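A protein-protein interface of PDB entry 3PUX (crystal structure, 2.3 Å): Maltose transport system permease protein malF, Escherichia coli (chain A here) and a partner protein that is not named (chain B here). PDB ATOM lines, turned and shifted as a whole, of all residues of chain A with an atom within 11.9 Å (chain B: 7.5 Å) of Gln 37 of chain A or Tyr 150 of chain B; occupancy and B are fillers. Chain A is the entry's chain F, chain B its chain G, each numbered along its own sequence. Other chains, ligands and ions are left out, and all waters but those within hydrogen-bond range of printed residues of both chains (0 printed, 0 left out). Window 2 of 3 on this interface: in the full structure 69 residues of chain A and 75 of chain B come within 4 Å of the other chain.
OE1 of Glu 39 of chain A is in salt-bridge range of NE of Arg 146 of chain B (3.5 Å). The side-chain carboxylate (OE2) of Glu 39 of chain A lies close to the side-chain carboxylate (OE2) of Glu 149 of chain B, 2.9 Å away.
The backbone carbonyl oxygen (O) of Leu 33 of chain A sits close to the side-chain amide oxygen (OE1) of Gln 37 of chain A. O of Met 34 of chain A sits close to N of Glu 39 of chain A (3.4 Å).
Leu 33 of chain A touches Tyr 150 of chain B. CG of Met 34 of chain A touches CZ of Tyr 150 of chain B, 3.6 Å away. OH of Tyr 150 of chain B touches NE2 of Gln 37 of chain A, at 3.8 Å. CG of Glu 39 of chain A touches OH of Tyr 150 of chain B (3.2 Å). Leu 143 of chain B touches Phe 42 of chain A. Arg 146 of chain B touches Phe 42 of chain A. CZ of Phe 42 of chain A touches CD1 of Leu 147 of chain B (3.9 Å). Leu 77 of chain A touches Leu 143 of chain B (O to CD2, 3.7 Å).
Val 27 of chain A touches none of the printed residues of chain B. Of the printed residues of chain B, Leu 33 of chain A touches Tyr 150 (3.6 Å). Printed residues of chain B within 4 Å of Met 34 of chain A: Tyr 150 (3.6 Å). Gln 37 of chain A touches just one residue of chain B: Tyr 150. Printed residues of chain B within 4 Å of Phe 42 of chain A: Leu 143, Arg 146 and Leu 147. Printed residues of chain A within 4 Å of Leu 143 of chain B: Phe 42 and Leu 77. Printed residues of chain A within 4 Å of Arg 146 of chain B: Glu 39 (3.1 Å) and Phe 42 (3.7 Å). No residue of chain A comes within 4 Å of Gly 148 of chain B. Of chain A, only Glu 39 comes within 4 Å of Glu 149 of chain B. Tyr 150 of chain B touches just these residues of chain A: Leu 33 (3.6 Å), Met 34 (3.6 Å), Gln 37 (3.8 Å) and Glu 39 (3.2 Å). No residue of chain A comes within 4 Å of Ile 151 of chain B. Pro 152 of chain B touches none of the printed residues of chain A. The nearest residue of chain B that does not touch Gln 37 of chain A is Glu 149 of chain B (4.8 Å).
Hydrophobic or aromatic side chains of chain A that line the printed part of chain B: Leu 33, Met 34 and Phe 42. Printed residues of chain B that touch a printed residue of chain A: Leu 143, Arg 146, Leu 147, Glu 149 and Tyr 150. Hydrophobic or aromatic side chains of chain B that line the printed part of chain A: Leu 143, Leu 147 and Tyr 150. Among the printed residues, 10 pairs touch across the chains.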
ATOM      1  N   LEU A  26      24.141  14.993 -10.346  1.00  0.00           N
ATOM      2  CA  LEU A  26      23.273  13.959 -10.917  1.00  0.00           C
ATOM      3  C   LEU A  26      22.451  13.325  -9.800  1.00  0.00           C
ATOM      4  O   LEU A  26      21.277  13.002  -9.984  1.00  0.00           O
ATOM      5  CB  LEU A  26      24.076  12.887 -11.658  1.00  0.00           C
ATOM      6  CG  LEU A  26      24.737  13.200 -13.004  1.00  0.00           C
ATOM      7  CD1 LEU A  26      25.193  11.899 -13.652  1.00  0.00           C
ATOM      8  CD2 LEU A  26      23.812  13.964 -13.952  1.00  0.00           C
ATOM      9  N   VAL A  27      23.082  13.155  -8.643  1.00  0.00           N
ATOM     10  CA  VAL A  27      22.375  12.870  -7.403  1.00  0.00           C
ATOM     11  C   VAL A  27      21.655  14.154  -6.986  1.00  0.00           C
ATOM     12  O   VAL A  27      22.286  15.192  -6.799  1.00  0.00           O
ATOM     13  CB  VAL A  27      23.350  12.405  -6.295  1.00  0.00           C
ATOM     14  CG1 VAL A  27      22.602  12.114  -4.996  1.00  0.00           C
ATOM     15  CG2 VAL A  27      24.126  11.175  -6.757  1.00  0.00           C
ATOM     16  N   GLY A  28      20.335  14.075  -6.850  1.00  0.00           N
ATOM     17  CA  GLY A  28      19.499  15.252  -6.611  1.00  0.00           C
ATOM     18  C   GLY A  28      18.637  15.483  -7.834  1.00  0.00           C
ATOM     19  O   GLY A  28      17.405  15.443  -7.761  1.00  0.00           O
ATOM     20  N   TYR A  29      19.301  15.712  -8.967  1.00  0.00           N
ATOM     21  CA  TYR A  29      18.649  15.802 -10.272  1.00  0.00           C
ATOM     22  C   TYR A  29      17.810  14.551 -10.512  1.00  0.00           C
ATOM     23  O   TYR A  29      16.739  14.619 -11.121  1.00  0.00           O
ATOM     24  CB  TYR A  29      19.703  15.966 -11.380  1.00  0.00           C
ATOM     25  CG  TYR A  29      19.164  16.075 -12.800  1.00  0.00           C
ATOM     26  CD1 TYR A  29      18.826  17.319 -13.350  1.00  0.00           C
ATOM     27  CD2 TYR A  29      19.017  14.937 -13.605  1.00  0.00           C
ATOM     28  CE1 TYR A  29      18.339  17.423 -14.662  1.00  0.00           C
ATOM     29  CE2 TYR A  29      18.530  15.029 -14.914  1.00  0.00           C
ATOM     30  CZ  TYR A  29      18.194  16.272 -15.436  1.00  0.00           C
ATOM     31  OH  TYR A  29      17.717  16.365 -16.725  1.00  0.00           O
ATOM     32  N   LEU A  30      18.311  13.417 -10.022  1.00  0.00           N
ATOM     33  CA  LEU A  30      17.616  12.142 -10.129  1.00  0.00           C
ATOM     34  C   LEU A  30      16.934  11.730  -8.819  1.00  0.00           C
ATOM     35  O   LEU A  30      16.144  10.792  -8.815  1.00  0.00           O
ATOM     36  CB  LEU A  30      18.570  11.037 -10.622  1.00  0.00           C
ATOM     37  CG  LEU A  30      19.003  10.998 -12.099  1.00  0.00           C
ATOM     38  CD1 LEU A  30      20.250  10.141 -12.294  1.00  0.00           C
ATOM     39  CD2 LEU A  30      17.885  10.507 -13.022  1.00  0.00           C
ATOM     40  N   VAL A  31      17.227  12.427  -7.721  1.00  0.00           N
ATOM     41  CA  VAL A  31      16.641  12.089  -6.414  1.00  0.00           C
ATOM     42  C   VAL A  31      15.349  12.858  -6.145  1.00  0.00           C
ATOM     43  O   VAL A  31      14.340  12.257  -5.761  1.00  0.00           O
ATOM     44  CB  VAL A  31      17.632  12.300  -5.237  1.00  0.00           C
ATOM     45  CG1 VAL A  31      16.934  12.107  -3.886  1.00  0.00           C
ATOM     46  CG2 VAL A  31      18.827  11.361  -5.360  1.00  0.00           C
ATOM     47  N   VAL A  32      15.386  14.179  -6.333  1.00  0.00           N
ATOM     48  CA  VAL A  32      14.192  15.025  -6.189  1.00  0.00           C
ATOM     49  C   VAL A  32      13.225  14.694  -7.332  1.00  0.00           C
ATOM     50  O   VAL A  32      12.008  14.779  -7.175  1.00  0.00           O
ATOM     51  CB  VAL A  32      14.536  16.548  -6.162  1.00  0.00           C
ATOM     52  CG1 VAL A  32      13.311  17.387  -5.780  1.00  0.00           C
ATOM     53  CG2 VAL A  32      15.678  16.833  -5.188  1.00  0.00           C
ATOM     54  N   LEU A  33      13.798  14.293  -8.467  1.00  0.00           N
ATOM     55  CA  LEU A  33      13.059  13.812  -9.632  1.00  0.00           C
ATOM     56  C   LEU A  33      12.376  12.462  -9.363  1.00  0.00           C
ATOM     57  O   LEU A  33      11.406  12.108 -10.032  1.00  0.00           O
ATOM     58  CB  LEU A  33      14.016  13.729 -10.829  1.00  0.00           C
ATOM     59  CG  LEU A  33      13.676  13.409 -12.294  1.00  0.00           C
ATOM     60  CD1 LEU A  33      13.904  11.948 -12.593  1.00  0.00           C
ATOM     61  CD2 LEU A  33      12.278  13.836 -12.720  1.00  0.00           C
ATOM     62  N   MET A  34      12.889  11.716  -8.386  1.00  0.00           N
ATOM     63  CA  MET A  34      12.244  10.492  -7.901  1.00  0.00           C
ATOM     64  C   MET A  34      11.198  10.824  -6.836  1.00  0.00           C
ATOM     65  O   MET A  34      10.259  10.054  -6.616  1.00  0.00           O
ATOM     66  CB  MET A  34      13.274   9.503  -7.332  1.00  0.00           C
ATOM     67  CG  MET A  34      13.988   8.634  -8.364  1.00  0.00           C
ATOM     68  SD  MET A  34      15.354   7.667  -7.663  1.00  0.00           S
ATOM     69  CE  MET A  34      16.137   7.057  -9.157  1.00  0.00           C
ATOM     70  N   TYR A  35      11.368  11.972  -6.178  1.00  0.00           N
ATOM     71  CA  TYR A  35      10.403  12.448  -5.189  1.00  0.00           C
ATOM     72  C   TYR A  35       9.076  12.800  -5.867  1.00  0.00           C
ATOM     73  O   TYR A  35       8.005  12.679  -5.263  1.00  0.00           O
ATOM     74  CB  TYR A  35      10.952  13.659  -4.431  1.00  0.00           C
ATOM     75  CG  TYR A  35      10.489  13.737  -2.993  1.00  0.00           C
ATOM     76  CD1 TYR A  35      11.218  13.122  -1.974  1.00  0.00           C
ATOM     77  CD2 TYR A  35       9.320  14.420  -2.650  1.00  0.00           C
ATOM     78  CE1 TYR A  35      10.799  13.182  -0.651  1.00  0.00           C
ATOM     79  CE2 TYR A  35       8.891  14.487  -1.326  1.00  0.00           C
ATOM     80  CZ  TYR A  35       9.637  13.865  -0.332  1.00  0.00           C
ATOM     81  OH  TYR A  35       9.228  13.926   0.983  1.00  0.00           O
ATOM     82  N   ALA A  36       9.167  13.225  -7.127  1.00  0.00           N
ATOM     83  CA  ALA A  36       7.998  13.500  -7.965  1.00  0.00           C
ATOM     84  C   ALA A  36       7.268  12.213  -8.374  1.00  0.00           C
ATOM     85  O   ALA A  36       7.720  11.107  -8.065  1.00  0.00           O
ATOM     86  CB  ALA A  36       8.405  14.310  -9.196  1.00  0.00           C
ATOM     87  N   GLN A  37       6.154  12.374  -9.091  1.00  0.00           N
ATOM     88  CA  GLN A  37       5.174  11.298  -9.388  1.00  0.00           C
ATOM     89  C   GLN A  37       4.804  10.379  -8.195  1.00  0.00           C
ATOM     90  O   GLN A  37       3.622  10.286  -7.830  1.00  0.00           O
ATOM     91  CB  GLN A  37       5.506  10.496 -10.680  1.00  0.00           C
ATOM     92  CG  GLN A  37       6.800   9.655 -10.690  1.00  0.00           C
ATOM     93  CD  GLN A  37       7.967  10.352 -11.382  1.00  0.00           C
ATOM     94  OE1 GLN A  37       8.460  11.384 -10.922  1.00  0.00           O
ATOM     95  NE2 GLN A  37       8.419   9.775 -12.493  1.00  0.00           N
ATOM     96  N   GLY A  38       5.809   9.728  -7.599  1.00  0.00           N
ATOM     97  CA  GLY A  38       5.614   8.855  -6.441  1.00  0.00           C
ATOM     98  C   GLY A  38       6.527   7.644  -6.466  1.00  0.00           C
ATOM     99  O   GLY A  38       6.130   6.565  -6.930  1.00  0.00           O
ATOM    100  N   GLU A  39       7.756   7.833  -5.980  1.00  0.00           N
ATOM    101  CA  GLU A  39       8.781   6.779  -5.925  1.00  0.00           C
ATOM    102  C   GLU A  39       9.623   7.016  -4.671  1.00  0.00           C
ATOM    103  O   GLU A  39      10.820   7.292  -4.761  1.00  0.00           O
ATOM    104  CB  GLU A  39       9.686   6.824  -7.168  1.00  0.00           C
ATOM    105  CG  GLU A  39       8.991   6.694  -8.524  1.00  0.00           C
ATOM    106  CD  GLU A  39       8.850   5.257  -8.998  1.00  0.00           C
ATOM    107  OE1 GLU A  39       9.236   4.325  -8.255  1.00  0.00           O
ATOM    108  OE2 GLU A  39       8.353   5.060 -10.127  1.00  0.00           O
ATOM    109  N   TYR A  40       8.994   6.907  -3.502  1.00  0.00           N
ATOM    110  CA  TYR A  40       9.601   7.373  -2.246  1.00  0.00           C
ATOM    111  C   TYR A  40      10.592   6.394  -1.614  1.00  0.00           C
ATOM    112  O   TYR A  40      11.674   6.793  -1.176  1.00  0.00           O
ATOM    113  CB  TYR A  40       8.516   7.797  -1.247  1.00  0.00           C
ATOM    114  CG  TYR A  40       7.689   8.965  -1.741  1.00  0.00           C
ATOM    115  CD1 TYR A  40       6.527   8.755  -2.487  1.00  0.00           C
ATOM    116  CD2 TYR A  40       8.077  10.280  -1.480  1.00  0.00           C
ATOM    117  CE1 TYR A  40       5.769   9.825  -2.949  1.00  0.00           C
ATOM    118  CE2 TYR A  40       7.325  11.357  -1.940  1.00  0.00           C
ATOM    119  CZ  TYR A  40       6.175  11.121  -2.672  1.00  0.00           C
ATOM    120  OH  TYR A  40       5.426  12.178  -3.129  1.00  0.00           O
ATOM    121  N   LEU A  41      10.214   5.119  -1.574  1.00  0.00           N
ATOM    122  CA  LEU A  41      11.109   4.050  -1.137  1.00  0.00           C
ATOM    123  C   LEU A  41      12.375   4.049  -1.996  1.00  0.00           C
ATOM    124  O   LEU A  41      13.467   3.784  -1.499  1.00  0.00           O
ATOM    125  CB  LEU A  41      10.393   2.692  -1.226  1.00  0.00           C
ATOM    126  CG  LEU A  41      10.843   1.484  -0.382  1.00  0.00           C
ATOM    127  CD1 LEU A  41       9.669   0.522  -0.180  1.00  0.00           C
ATOM    128  CD2 LEU A  41      12.042   0.743  -0.977  1.00  0.00           C
ATOM    129  N   PHE A  42      12.218   4.379  -3.278  1.00  0.00           N
ATOM    130  CA  PHE A  42      13.321   4.408  -4.234  1.00  0.00           C
ATOM    131  C   PHE A  42      14.143   5.699  -4.180  1.00  0.00           C
ATOM    132  O   PHE A  42      15.198   5.790  -4.801  1.00  0.00           O
ATOM    133  CB  PHE A  42      12.790   4.188  -5.650  1.00  0.00           C
ATOM    134  CG  PHE A  42      13.759   3.492  -6.559  1.00  0.00           C
ATOM    135  CD1 PHE A  42      14.675   4.221  -7.317  1.00  0.00           C
ATOM    136  CD2 PHE A  42      13.756   2.105  -6.660  1.00  0.00           C
ATOM    137  CE1 PHE A  42      15.579   3.583  -8.163  1.00  0.00           C
ATOM    138  CE2 PHE A  42      14.654   1.455  -7.502  1.00  0.00           C
ATOM    139  CZ  PHE A  42      15.570   2.197  -8.259  1.00  0.00           C
ATOM    140  N   ALA A  43      13.658   6.693  -3.444  1.00  0.00           N
ATOM    141  CA  ALA A  43      14.383   7.948  -3.277  1.00  0.00           C
ATOM    142  C   ALA A  43      15.229   7.930  -2.004  1.00  0.00           C
ATOM    143  O   ALA A  43      16.384   8.363  -2.012  1.00  0.00           O
ATOM    144  CB  ALA A  43      13.421   9.124  -3.266  1.00  0.00           C
ATOM    145  N   ILE A  44      14.643   7.431  -0.915  1.00  0.00           N
ATOM    146  CA  ILE A  44      15.336   7.302   0.372  1.00  0.00           C
ATOM    147  C   ILE A  44      16.496   6.324   0.223  1.00  0.00           C
ATOM    148  O   ILE A  44      17.596   6.571   0.723  1.00  0.00           O
ATOM    149  CB  ILE A  44      14.371   6.828   1.507  1.00  0.00           C
ATOM    150  CG1 ILE A  44      13.266   7.872   1.749  1.00  0.00           C
ATOM    151  CG2 ILE A  44      15.143   6.523   2.804  1.00  0.00           C
ATOM    152  CD1 ILE A  44      12.033   7.348   2.497  1.00  0.00           C
ATOM    153  N   THR A  45      16.245   5.229  -0.489  1.00  0.00           N
ATOM    154  CA  THR A  45      17.237   4.173  -0.655  1.00  0.00           C
ATOM    155  C   THR A  45      18.441   4.656  -1.481  1.00  0.00           C
ATOM    156  O   THR A  45      19.590   4.332  -1.170  1.00  0.00           O
ATOM    157  CB  THR A  45      16.588   2.860  -1.219  1.00  0.00           C
ATOM    158  OG1 THR A  45      17.192   1.711  -0.609  1.00  0.00           O
ATOM    159  CG2 THR A  45      16.682   2.757  -2.754  1.00  0.00           C
ATOM    160  N   THR A  46      18.167   5.462  -2.503  1.00  0.00           N
ATOM    161  CA  THR A  46      19.186   5.920  -3.435  1.00  0.00           C
ATOM    162  C   THR A  46      19.957   7.122  -2.868  1.00  0.00           C
ATOM    163  O   THR A  46      21.038   7.466  -3.349  1.00  0.00           O
ATOM    164  CB  THR A  46      18.556   6.208  -4.830  1.00  0.00           C
ATOM    165  OG1 THR A  46      19.512   5.971  -5.866  1.00  0.00           O
ATOM    166  CG2 THR A  46      18.041   7.625  -4.933  1.00  0.00           C
ATOM    167  N   LEU A  47      19.401   7.743  -1.829  1.00  0.00           N
ATOM    168  CA  LEU A  47      20.055   8.863  -1.161  1.00  0.00           C
ATOM    169  C   LEU A  47      21.194   8.376  -0.262  1.00  0.00           C
ATOM    170  O   LEU A  47      22.327   8.850  -0.384  1.00  0.00           O
ATOM    171  CB  LEU A  47      19.051   9.698  -0.349  1.00  0.00           C
ATOM    172  CG  LEU A  47      19.606  10.976   0.302  1.00  0.00           C
ATOM    173  CD1 LEU A  47      19.269  12.208  -0.534  1.00  0.00           C
ATOM    174  CD2 LEU A  47      19.115  11.141   1.740  1.00  0.00           C
ATOM    175  N   SER A  50      24.142   6.792  -2.500  1.00  0.00           N
ATOM    176  CA  SER A  50      24.982   7.753  -3.232  1.00  0.00           C
ATOM    177  C   SER A  50      25.814   8.623  -2.296  1.00  0.00           C
ATOM    178  O   SER A  50      26.972   8.936  -2.587  1.00  0.00           O
ATOM    179  CB  SER A  50      24.125   8.652  -4.117  1.00  0.00           C
ATOM    180  OG  SER A  50      23.496   7.912  -5.144  1.00  0.00           O
ATOM    181  N   LEU A  77      22.112  -4.308  -3.500  1.00  0.00           N
ATOM    182  CA  LEU A  77      21.108  -4.091  -4.532  1.00  0.00           C
ATOM    183  C   LEU A  77      20.437  -5.360  -5.057  1.00  0.00           C
ATOM    184  O   LEU A  77      19.219  -5.386  -5.223  1.00  0.00           O
ATOM    185  CB  LEU A  77      21.728  -3.324  -5.698  1.00  0.00           C
ATOM    186  CG  LEU A  77      20.899  -2.221  -6.352  1.00  0.00           C
ATOM    187  CD1 LEU A  77      20.264  -1.274  -5.292  1.00  0.00           C
ATOM    188  CD2 LEU A  77      21.786  -1.433  -7.324  1.00  0.00           C
ATOM    189  N   LEU B 143      12.370  -3.944  -9.330  1.00  0.00           N
ATOM    190  CA  LEU B 143      13.544  -3.101  -9.259  1.00  0.00           C
ATOM    191  C   LEU B 143      13.923  -2.536 -10.623  1.00  0.00           C
ATOM    192  O   LEU B 143      14.047  -1.323 -10.787  1.00  0.00           O
ATOM    193  CB  LEU B 143      14.725  -3.862  -8.630  1.00  0.00           C
ATOM    194  CG  LEU B 143      16.059  -3.124  -8.537  1.00  0.00           C
ATOM    195  CD1 LEU B 143      15.877  -1.859  -7.758  1.00  0.00           C
ATOM    196  CD2 LEU B 143      17.142  -3.983  -7.894  1.00  0.00           C
ATOM    197  N   PHE B 144      14.107  -3.411 -11.602  1.00  0.00           N
ATOM    198  CA  PHE B 144      14.540  -2.966 -12.918  1.00  0.00           C
ATOM    199  C   PHE B 144      13.438  -2.235 -13.683  1.00  0.00           C
ATOM    200  O   PHE B 144      13.716  -1.538 -14.662  1.00  0.00           O
ATOM    201  CB  PHE B 144      15.034  -4.134 -13.730  1.00  0.00           C
ATOM    202  CG  PHE B 144      16.408  -4.575 -13.377  1.00  0.00           C
ATOM    203  CD1 PHE B 144      16.607  -5.651 -12.524  1.00  0.00           C
ATOM    204  CD2 PHE B 144      17.511  -3.934 -13.922  1.00  0.00           C
ATOM    205  CE1 PHE B 144      17.905  -6.072 -12.215  1.00  0.00           C
ATOM    206  CE2 PHE B 144      18.792  -4.342 -13.627  1.00  0.00           C
ATOM    207  CZ  PHE B 144      18.998  -5.407 -12.775  1.00  0.00           C
ATOM    208  N   ASP B 145      12.196  -2.398 -13.240  1.00  0.00           N
ATOM    209  CA  ASP B 145      11.090  -1.640 -13.809  1.00  0.00           C
ATOM    210  C   ASP B 145      11.249  -0.176 -13.409  1.00  0.00           C
ATOM    211  O   ASP B 145      11.144   0.724 -14.248  1.00  0.00           O
ATOM    212  CB  ASP B 145       9.736  -2.197 -13.338  1.00  0.00           C
ATOM    213  CG  ASP B 145       8.570  -1.762 -14.227  1.00  0.00           C
ATOM    214  OD1 ASP B 145       8.803  -1.108 -15.274  1.00  0.00           O
ATOM    215  OD2 ASP B 145       7.405  -2.082 -13.883  1.00  0.00           O
ATOM    216  N   ARG B 146      11.515   0.040 -12.122  1.00  0.00           N
ATOM    217  CA  ARG B 146      11.710   1.369 -11.566  1.00  0.00           C
ATOM    218  C   ARG B 146      12.924   2.022 -12.203  1.00  0.00           C
ATOM    219  O   ARG B 146      12.850   3.135 -12.707  1.00  0.00           O
ATOM    220  CB  ARG B 146      11.905   1.296 -10.043  1.00  0.00           C
ATOM    221  CG  ARG B 146      10.695   1.723  -9.211  1.00  0.00           C
ATOM    222  CD  ARG B 146       9.804   0.547  -8.808  1.00  0.00           C
ATOM    223  NE  ARG B 146       8.442   0.965  -8.465  1.00  0.00           N
ATOM    224  CZ  ARG B 146       7.430   0.130  -8.240  1.00  0.00           C
ATOM    225  NH1 ARG B 146       7.621  -1.185  -8.311  1.00  0.00           N
ATOM    226  NH2 ARG B 146       6.220   0.606  -7.950  1.00  0.00           N
ATOM    227  N   LEU B 147      14.037   1.305 -12.179  1.00  0.00           N
ATOM    228  CA  LEU B 147      15.324   1.803 -12.651  1.00  0.00           C
ATOM    229  C   LEU B 147      15.264   2.269 -14.097  1.00  0.00           C
ATOM    230  O   LEU B 147      15.887   3.273 -14.471  1.00  0.00           O
ATOM    231  CB  LEU B 147      16.358   0.686 -12.520  1.00  0.00           C
ATOM    232  CG  LEU B 147      17.831   1.045 -12.421  1.00  0.00           C
ATOM    233  CD1 LEU B 147      18.114   1.953 -11.224  1.00  0.00           C
ATOM    234  CD2 LEU B 147      18.618  -0.256 -12.317  1.00  0.00           C
ATOM    235  N   GLY B 148      14.491   1.529 -14.887  1.00  0.00           N
ATOM    236  CA  GLY B 148      14.413   1.707 -16.327  1.00  0.00           C
ATOM    237  C   GLY B 148      14.020   3.095 -16.771  1.00  0.00           C
ATOM    238  O   GLY B 148      14.521   3.595 -17.774  1.00  0.00           O
ATOM    239  N   GLU B 149      13.125   3.727 -16.023  1.00  0.00           N
ATOM    240  CA  GLU B 149      12.643   5.049 -16.393  1.00  0.00           C
ATOM    241  C   GLU B 149      13.633   6.155 -16.058  1.00  0.00           C
ATOM    242  O   GLU B 149      13.473   7.279 -16.518  1.00  0.00           O
ATOM    243  CB  GLU B 149      11.268   5.318 -15.788  1.00  0.00           C
ATOM    244  CG  GLU B 149      11.136   5.050 -14.294  1.00  0.00           C
ATOM    245  CD  GLU B 149       9.729   4.590 -13.911  1.00  0.00           C
ATOM    246  OE1 GLU B 149       9.147   3.771 -14.663  1.00  0.00           O
ATOM    247  OE2 GLU B 149       9.204   5.040 -12.865  1.00  0.00           O
ATOM    248  N   TYR B 150      14.668   5.829 -15.285  1.00  0.00           N
ATOM    249  CA  TYR B 150      15.720   6.792 -14.959  1.00  0.00           C
ATOM    250  C   TYR B 150      17.015   6.526 -15.751  1.00  0.00           C
ATOM    251  O   TYR B 150      17.554   7.436 -16.386  1.00  0.00           O
ATOM    252  CB  TYR B 150      15.947   6.841 -13.439  1.00  0.00           C
ATOM    253  CG  TYR B 150      14.653   7.079 -12.683  1.00  0.00           C
ATOM    254  CD1 TYR B 150      14.040   6.055 -11.958  1.00  0.00           C
ATOM    255  CD2 TYR B 150      14.016   8.322 -12.732  1.00  0.00           C
ATOM    256  CE1 TYR B 150      12.833   6.274 -11.275  1.00  0.00           C
ATOM    257  CE2 TYR B 150      12.813   8.550 -12.062  1.00  0.00           C
ATOM    258  CZ  TYR B 150      12.225   7.529 -11.337  1.00  0.00           C
ATOM    259  OH  TYR B 150      11.038   7.774 -10.676  1.00  0.00           O
ATOM    260  N   ILE B 151      17.500   5.284 -15.719  1.00  0.00           N
ATOM    261  CA  ILE B 151      18.602   4.863 -16.588  1.00  0.00           C
ATOM    262  C   ILE B 151      18.086   3.738 -17.489  1.00  0.00           C
ATOM    263  O   ILE B 151      18.182   2.572 -17.132  1.00  0.00           O
ATOM    264  CB  ILE B 151      19.851   4.382 -15.792  1.00  0.00           C
ATOM    265  CG1 ILE B 151      20.188   5.320 -14.626  1.00  0.00           C
ATOM    266  CG2 ILE B 151      21.074   4.207 -16.716  1.00  0.00           C
ATOM    267  CD1 ILE B 151      19.942   4.719 -13.250  1.00  0.00           C
ATOM    268  N   PRO B 152      17.523   4.082 -18.662  1.00  0.00           N
ATOM    269  CA  PRO B 152      16.924   3.053 -19.518  1.00  0.00           C
ATOM    270  C   PRO B 152      17.919   2.036 -20.077  1.00  0.00           C
ATOM    271  O   PRO B 152      17.500   0.985 -20.532  1.00  0.00           O
ATOM    272  CB  PRO B 152      16.291   3.862 -20.662  1.00  0.00           C
ATOM    273  CG  PRO B 152      16.212   5.263 -20.154  1.00  0.00           C
ATOM    274  CD  PRO B 152      17.393   5.422 -19.258  1.00  0.00           C
ATOM    275  N   PHE B 153      19.210   2.355 -20.028  1.00  0.00           N
ATOM    276  CA  PHE B 153      20.287   1.479 -20.497  1.00  0.00           C
ATOM    277  C   PHE B 153      20.399   0.207 -19.643  1.00  0.00           C
ATOM    278  O   PHE B 153      20.887  -0.840 -20.103  1.00  0.00           O
ATOM    279  CB  PHE B 153      21.612   2.267 -20.473  1.00  0.00           C
ATOM    280  CG  PHE B 153      22.687   1.710 -21.386  1.00  0.00           C
ATOM    281  CD1 PHE B 153      22.375   1.254 -22.681  1.00  0.00           C
ATOM    282  CD2 PHE B 153      24.026   1.664 -20.961  1.00  0.00           C
ATOM    283  CE1 PHE B 153      23.376   0.733 -23.536  1.00  0.00           C
ATOM    284  CE2 PHE B 153      25.045   1.150 -21.808  1.00  0.00           C
ATOM    285  CZ  PHE B 153      24.710   0.688 -23.101  1.00  0.00           C
ATOM    286  N   ILE B 154      19.943   0.299 -18.398  1.00  0.00           N
ATOM    287  CA  ILE B 154      19.982  -0.840 -17.480  1.00  0.00           C
ATOM    288  C   ILE B 154      18.598  -1.225 -16.977  1.00  0.00           C
ATOM    289  O   ILE B 154      18.469  -1.814 -15.914  1.00  0.00           O
ATOM    290  CB  ILE B 154      20.933  -0.582 -16.268  1.00  0.00           C
ATOM    291  CG1 ILE B 154      20.490   0.666 -15.478  1.00  0.00           C
ATOM    292  CG2 ILE B 154      22.400  -0.515 -16.738  1.00  0.00           C
ATOM    293  CD1 ILE B 154      21.441   1.082 -14.368  1.00  0.00           C
